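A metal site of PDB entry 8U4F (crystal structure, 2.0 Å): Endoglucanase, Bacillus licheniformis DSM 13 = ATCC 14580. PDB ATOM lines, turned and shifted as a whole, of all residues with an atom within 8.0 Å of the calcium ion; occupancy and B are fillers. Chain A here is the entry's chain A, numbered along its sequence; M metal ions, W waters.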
ATOM      1  N   LEU A  66     -10.219 -11.100  -3.749  1.00  0.00           N
ATOM      2  CA  LEU A  66      -9.477 -11.398  -2.527  1.00  0.00           C
ATOM      3  C   LEU A  66     -10.402 -11.758  -1.384  1.00  0.00           C
ATOM      4  O   LEU A  66     -10.243 -12.847  -0.804  1.00  0.00           O
ATOM      5  CB  LEU A  66      -8.524 -10.250  -2.177  1.00  0.00           C
ATOM      6  CG  LEU A  66      -7.644 -10.465  -0.938  1.00  0.00           C
ATOM      7  CD1 LEU A  66      -6.542 -11.490  -1.197  1.00  0.00           C
ATOM      8  CD2 LEU A  66      -7.032  -9.155  -0.448  1.00  0.00           C
ATOM      9  N   SER A 152       0.448 -12.110  -5.397  1.00  0.00           N
ATOM     10  CA  SER A 152       0.703 -13.275  -4.544  1.00  0.00           C
ATOM     11  C   SER A 152      -0.358 -13.414  -3.458  1.00  0.00           C
ATOM     12  O   SER A 152      -0.665 -14.537  -3.046  1.00  0.00           O
ATOM     13  CB  SER A 152       2.107 -13.174  -3.935  1.00  0.00           C
ATOM     14  OG  SER A 152       3.092 -12.958  -4.933  1.00  0.00           O
ATOM     15  N   ASP A 153      -0.928 -12.305  -2.985  1.00  0.00           N
ATOM     16  CA  ASP A 153      -2.019 -12.386  -2.025  1.00  0.00           C
ATOM     17  C   ASP A 153      -3.261 -13.004  -2.655  1.00  0.00           C
ATOM     18  O   ASP A 153      -3.840 -13.952  -2.108  1.00  0.00           O
ATOM     19  CB  ASP A 153      -2.326 -11.009  -1.436  1.00  0.00           C
ATOM     20  CG  ASP A 153      -2.043  -9.870  -2.415  1.00  0.00           C
ATOM     21  OD1 ASP A 153      -2.177 -10.060  -3.647  1.00  0.00           O
ATOM     22  OD2 ASP A 153      -1.647  -8.789  -1.933  1.00  0.00           O
ATOM     23  N   LEU A 154      -3.685 -12.479  -3.810  1.00  0.00           N
ATOM     24  CA  LEU A 154      -4.877 -13.016  -4.449  1.00  0.00           C
ATOM     25  C   LEU A 154      -4.675 -14.476  -4.865  1.00  0.00           C
ATOM     26  O   LEU A 154      -5.508 -15.337  -4.558  1.00  0.00           O
ATOM     27  CB  LEU A 154      -5.239 -12.159  -5.664  1.00  0.00           C
ATOM     28  CG  LEU A 154      -6.466 -12.638  -6.466  1.00  0.00           C
ATOM     29  CD1 LEU A 154      -7.701 -12.630  -5.589  1.00  0.00           C
ATOM     30  CD2 LEU A 154      -6.702 -11.755  -7.695  1.00  0.00           C
ATOM     31  N   LYS A 197       1.794  -7.388  -4.732  1.00  0.00           N
ATOM     32  CA  LYS A 197       0.447  -7.193  -4.209  1.00  0.00           C
ATOM     33  C   LYS A 197      -0.548  -7.057  -5.363  1.00  0.00           C
ATOM     34  O   LYS A 197      -0.336  -6.262  -6.284  1.00  0.00           O
ATOM     35  CB  LYS A 197       0.387  -5.950  -3.326  1.00  0.00           C
ATOM     36  CG  LYS A 197       1.330  -6.038  -2.129  1.00  0.00           C
ATOM     37  CD  LYS A 197       1.112  -4.890  -1.148  1.00  0.00           C
ATOM     38  CE  LYS A 197       1.508  -3.572  -1.761  1.00  0.00           C
ATOM     39  NZ  LYS A 197       1.170  -2.453  -0.837  1.00  0.00           N
ATOM     40  N   ASN A 210      -7.884  -2.987  -0.578  1.00  0.00           N
ATOM     41  CA  ASN A 210      -6.453  -2.759  -0.642  1.00  0.00           C
ATOM     42  C   ASN A 210      -5.687  -3.838   0.118  1.00  0.00           C
ATOM     43  O   ASN A 210      -6.124  -4.324   1.168  1.00  0.00           O
ATOM     44  CB  ASN A 210      -6.148  -1.373  -0.065  1.00  0.00           C
ATOM     45  CG  ASN A 210      -4.696  -0.954  -0.277  1.00  0.00           C
ATOM     46  OD1 ASN A 210      -4.130  -1.154  -1.349  1.00  0.00           O
ATOM     47  ND2 ASN A 210      -4.092  -0.368   0.743  1.00  0.00           N
ATOM     48  N   SER A 211      -4.534  -4.225  -0.420  1.00  0.00           N
ATOM     49  CA  SER A 211      -3.671  -5.210   0.249  1.00  0.00           C
ATOM     50  C   SER A 211      -2.852  -4.488   1.324  1.00  0.00           C
ATOM     51  O   SER A 211      -1.668  -4.172   1.148  1.00  0.00           O
ATOM     52  CB  SER A 211      -2.794  -5.943  -0.746  1.00  0.00           C
ATOM     53  OG  SER A 211      -2.068  -6.962  -0.078  1.00  0.00           O
ATOM     54  N   TRP A 212      -3.521  -4.221   2.440  1.00  0.00           N
ATOM     55  CA  TRP A 212      -2.894  -3.497   3.538  1.00  0.00           C
ATOM     56  C   TRP A 212      -1.698  -4.265   4.092  1.00  0.00           C
ATOM     57  O   TRP A 212      -0.627  -3.681   4.302  1.00  0.00           O
ATOM     58  CB  TRP A 212      -3.917  -3.254   4.638  1.00  0.00           C
ATOM     59  CG  TRP A 212      -5.120  -2.503   4.179  1.00  0.00           C
ATOM     60  CD1 TRP A 212      -6.357  -3.020   3.899  1.00  0.00           C
ATOM     61  CD2 TRP A 212      -5.211  -1.095   3.944  1.00  0.00           C
ATOM     62  NE1 TRP A 212      -7.214  -2.009   3.496  1.00  0.00           N
ATOM     63  CE2 TRP A 212      -6.530  -0.819   3.519  1.00  0.00           C
ATOM     64  CE3 TRP A 212      -4.304  -0.041   4.039  1.00  0.00           C
ATOM     65  CZ2 TRP A 212      -6.967   0.464   3.203  1.00  0.00           C
ATOM     66  CZ3 TRP A 212      -4.738   1.250   3.717  1.00  0.00           C
ATOM     67  CH2 TRP A 212      -6.055   1.476   3.314  1.00  0.00           C
ATOM     68  N   SER A 213      -1.853  -5.558   4.323  1.00  0.00           N
ATOM     69  CA  SER A 213      -0.843  -6.359   4.994  1.00  0.00           C
ATOM     70  C   SER A 213       0.189  -6.966   4.048  1.00  0.00           C
ATOM     71  O   SER A 213       1.108  -7.637   4.523  1.00  0.00           O
ATOM     72  CB  SER A 213      -1.512  -7.489   5.777  1.00  0.00           C
ATOM     73  OG  SER A 213      -2.142  -8.403   4.894  1.00  0.00           O
ATOM     74  N   GLY A 214       0.064  -6.755   2.737  1.00  0.00           N
ATOM     75  CA  GLY A 214       0.968  -7.412   1.806  1.00  0.00           C
ATOM     76  C   GLY A 214       0.625  -8.888   1.649  1.00  0.00           C
ATOM     77  O   GLY A 214      -0.407  -9.368   2.125  1.00  0.00           O
ATOM     78  N   TYR A 215       1.518  -9.620   0.977  1.00  0.00           N
ATOM     79  CA  TYR A 215       1.236 -10.982   0.531  1.00  0.00           C
ATOM     80  C   TYR A 215       1.955 -12.058   1.326  1.00  0.00           C
ATOM     81  O   TYR A 215       1.708 -13.247   1.080  1.00  0.00           O
ATOM     82  CB  TYR A 215       1.583 -11.135  -0.961  1.00  0.00           C
ATOM     83  CG  TYR A 215       2.991 -10.731  -1.336  1.00  0.00           C
ATOM     84  CD1 TYR A 215       4.084 -11.566  -1.060  1.00  0.00           C
ATOM     85  CD2 TYR A 215       3.241  -9.523  -1.973  1.00  0.00           C
ATOM     86  CE1 TYR A 215       5.380 -11.189  -1.418  1.00  0.00           C
ATOM     87  CE2 TYR A 215       4.537  -9.146  -2.331  1.00  0.00           C
ATOM     88  CZ  TYR A 215       5.590  -9.973  -2.043  1.00  0.00           C
ATOM     89  OH  TYR A 215       6.860  -9.592  -2.408  1.00  0.00           O
ATOM     90  N   LYS A 216       2.827 -11.687   2.261  1.00  0.00           N
ATOM     91  CA  LYS A 216       3.601 -12.702   2.972  1.00  0.00           C
ATOM     92  C   LYS A 216       2.706 -13.653   3.759  1.00  0.00           C
ATOM     93  O   LYS A 216       3.037 -14.824   3.900  1.00  0.00           O
ATOM     94  CB  LYS A 216       4.617 -12.019   3.889  1.00  0.00           C
ATOM     95  CG  LYS A 216       5.879 -11.633   3.124  1.00  0.00           C
ATOM     96  CD  LYS A 216       6.597 -10.400   3.678  1.00  0.00           C
ATOM     97  CE  LYS A 216       7.797 -10.038   2.782  1.00  0.00           C
ATOM     98  NZ  LYS A 216       7.400  -9.946   1.346  1.00  0.00           N
ATOM     99  N   ASP A 217       1.567 -13.170   4.241  1.00  0.00           N
ATOM    100  CA  ASP A 217       0.671 -14.052   4.982  1.00  0.00           C
ATOM    101  C   ASP A 217      -0.046 -15.038   4.066  1.00  0.00           C
ATOM    102  O   ASP A 217      -0.248 -16.203   4.432  1.00  0.00           O
ATOM    103  CB  ASP A 217      -0.323 -13.226   5.806  1.00  0.00           C
ATOM    104  CG  ASP A 217      -0.972 -12.104   5.017  1.00  0.00           C
ATOM    105  OD1 ASP A 217      -0.242 -11.291   4.407  1.00  0.00           O
ATOM    106  OD2 ASP A 217      -2.207 -12.023   5.012  1.00  0.00           O
ATOM    107  N   GLU A 218      -0.430 -14.614   2.861  1.00  0.00           N
ATOM    108  CA  GLU A 218      -1.124 -15.529   1.947  1.00  0.00           C
ATOM    109  C   GLU A 218      -0.190 -16.612   1.427  1.00  0.00           C
ATOM    110  O   GLU A 218      -0.628 -17.737   1.200  1.00  0.00           O
ATOM    111  CB  GLU A 218      -1.758 -14.774   0.785  1.00  0.00           C
ATOM    112  CG  GLU A 218      -3.043 -14.029   1.157  1.00  0.00           C
ATOM    113  CD  GLU A 218      -2.766 -12.672   1.770  1.00  0.00           C
ATOM    114  OE1 GLU A 218      -1.580 -12.336   1.973  1.00  0.00           O
ATOM    115  OE2 GLU A 218      -3.726 -11.928   2.043  1.00  0.00           O
ATOM    116  N   LEU A 219       1.098 -16.297   1.227  1.00  0.00           N
ATOM    117  CA  LEU A 219       2.046 -17.330   0.834  1.00  0.00           C
ATOM    118  C   LEU A 219       2.126 -18.441   1.874  1.00  0.00           C
ATOM    119  O   LEU A 219       2.164 -19.625   1.516  1.00  0.00           O
ATOM    120  CB  LEU A 219       3.435 -16.706   0.610  1.00  0.00           C
ATOM    121  CG  LEU A 219       3.575 -15.756  -0.587  1.00  0.00           C
ATOM    122  CD1 LEU A 219       4.980 -15.160  -0.648  1.00  0.00           C
ATOM    123  CD2 LEU A 219       3.217 -16.460  -1.885  1.00  0.00           C
ATOM    124  N   SER A 259      -8.718 -11.953   9.007  1.00  0.00           N
ATOM    125  CA  SER A 259      -9.549 -11.120   8.145  1.00  0.00           C
ATOM    126  C   SER A 259      -9.248 -11.420   6.678  1.00  0.00           C
ATOM    127  O   SER A 259      -8.282 -12.117   6.350  1.00  0.00           O
ATOM    128  CB  SER A 259      -9.324  -9.623   8.435  1.00  0.00           C
ATOM    129  OG  SER A 259      -7.987  -9.245   8.167  1.00  0.00           O
ATOM    130  N   TRP A 260     -10.099 -10.876   5.796  1.00  0.00           N
ATOM    131  CA  TRP A 260      -9.876 -11.046   4.365  1.00  0.00           C
ATOM    132  C   TRP A 260      -8.517 -10.534   3.922  1.00  0.00           C
ATOM    133  O   TRP A 260      -8.010 -10.969   2.889  1.00  0.00           O
ATOM    134  CB  TRP A 260     -10.958 -10.321   3.557  1.00  0.00           C
ATOM    135  CG  TRP A 260     -11.017  -8.837   3.826  1.00  0.00           C
ATOM    136  CD1 TRP A 260     -11.851  -8.202   4.689  1.00  0.00           C
ATOM    137  CD2 TRP A 260     -10.196  -7.820   3.237  1.00  0.00           C
ATOM    138  NE1 TRP A 260     -11.606  -6.858   4.674  1.00  0.00           N
ATOM    139  CE2 TRP A 260     -10.591  -6.594   3.791  1.00  0.00           C
ATOM    140  CE3 TRP A 260      -9.174  -7.829   2.280  1.00  0.00           C
ATOM    141  CZ2 TRP A 260      -9.994  -5.381   3.439  1.00  0.00           C
ATOM    142  CZ3 TRP A 260      -8.578  -6.616   1.928  1.00  0.00           C
ATOM    143  CH2 TRP A 260      -8.991  -5.416   2.508  1.00  0.00           C
ATOM    144  N   ASP A 261      -7.913  -9.608   4.671  1.00  0.00           N
ATOM    145  CA  ASP A 261      -6.615  -9.063   4.299  1.00  0.00           C
ATOM    146  C   ASP A 261      -5.457  -9.762   4.983  1.00  0.00           C
ATOM    147  O   ASP A 261      -4.384  -9.881   4.389  1.00  0.00           O
ATOM    148  CB  ASP A 261      -6.518  -7.567   4.618  1.00  0.00           C
ATOM    149  CG  ASP A 261      -5.238  -6.957   4.081  1.00  0.00           C
ATOM    150  OD1 ASP A 261      -5.103  -6.900   2.835  1.00  0.00           O
ATOM    151  OD2 ASP A 261      -4.378  -6.541   4.895  1.00  0.00           O
ATOM    152  N   ASP A 262      -5.628 -10.206   6.227  1.00  0.00           N
ATOM    153  CA  ASP A 262      -4.527 -10.749   7.013  1.00  0.00           C
ATOM    154  C   ASP A 262      -4.888 -12.148   7.478  1.00  0.00           C
ATOM    155  O   ASP A 262      -5.690 -12.326   8.400  1.00  0.00           O
ATOM    156  CB  ASP A 262      -4.192  -9.844   8.191  1.00  0.00           C
ATOM    157  CG  ASP A 262      -2.794 -10.085   8.714  1.00  0.00           C
ATOM    158  OD1 ASP A 262      -2.298 -11.230   8.528  1.00  0.00           O
ATOM    159  OD2 ASP A 262      -2.189  -9.151   9.283  1.00  0.00           O
ATOM    160  N   VAL A 263      -4.269 -13.155   6.851  1.00  0.00           N
ATOM    161  CA  VAL A 263      -4.489 -14.544   7.218  1.00  0.00           C
ATOM    162  C   VAL A 263      -3.333 -15.105   8.039  1.00  0.00           C
ATOM    163  O   VAL A 263      -3.239 -16.326   8.234  1.00  0.00           O
ATOM    164  CB  VAL A 263      -4.740 -15.412   5.972  1.00  0.00           C
ATOM    165  CG1 VAL A 263      -6.149 -15.177   5.434  1.00  0.00           C
ATOM    166  CG2 VAL A 263      -3.703 -15.108   4.906  1.00  0.00           C
ATOM    167  N   THR A 264      -2.429 -14.241   8.522  1.00  0.00           N
ATOM    168  CA  THR A 264      -1.404 -14.673   9.460  1.00  0.00           C
ATOM    169  C   THR A 264      -2.036 -15.462  10.603  1.00  0.00           C
ATOM    170  O   THR A 264      -1.556 -16.540  10.974  1.00  0.00           O
ATOM    171  CB  THR A 264      -0.649 -13.468  10.027  1.00  0.00           C
ATOM    172  OG1 THR A 264      -0.086 -12.685   8.967  1.00  0.00           O
ATOM    173  CG2 THR A 264       0.456 -13.913  10.965  1.00  0.00           C
HETATM  174 CA    CA M   1      -2.291 -10.251   3.279  1.00  0.00          CA
HETATM  175  O   HOH W   1      -3.099  -8.461   1.897  1.00  0.00           O
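Water W1 lies within hydrogen-bond range of OG of Ser 211 and OD1 of Asp 261.
The calcium ion is bound by O of Gly 214 (2.4 Å). O of Asp 261 binds the calcium ion (2.4 Å). The calcium ion is bound by water W1, 2.4 Å away. The calcium ion is bound by the side-chain hydroxyl (OG) of Ser 213 (2.5 Å). The calcium ion is bound by the side-chain carboxylate (OD2) of Asp 217 (2.5 Å). OE2 of Glu 218 is bound to the calcium ion, at 2.5 Å. The side-chain carboxylate (OD1) of Asp 217 is bound to the calcium ion, at 2.6 Å. The side-chain carboxylate (OE1) of Glu 218 binds the calcium ion, 2.6 Å away.
The side-chain carboxylate (OD1) of Asp 261 lies within hydrogen-bond range of the backbone NH (N) of Trp 212, at 3.1 Å. The backbone NH (N) of Val 263 sits close to the side-chain carboxylate (OD2) of Asp 217, 3.0 Å away.
Within 4 Å of the calcium ion: Ser 213, Gly 214, Asp 217, Glu 218 and Asp 261. The nearest printed residue that does not touch the calcium ion is Asp 262 (4.4 Å).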
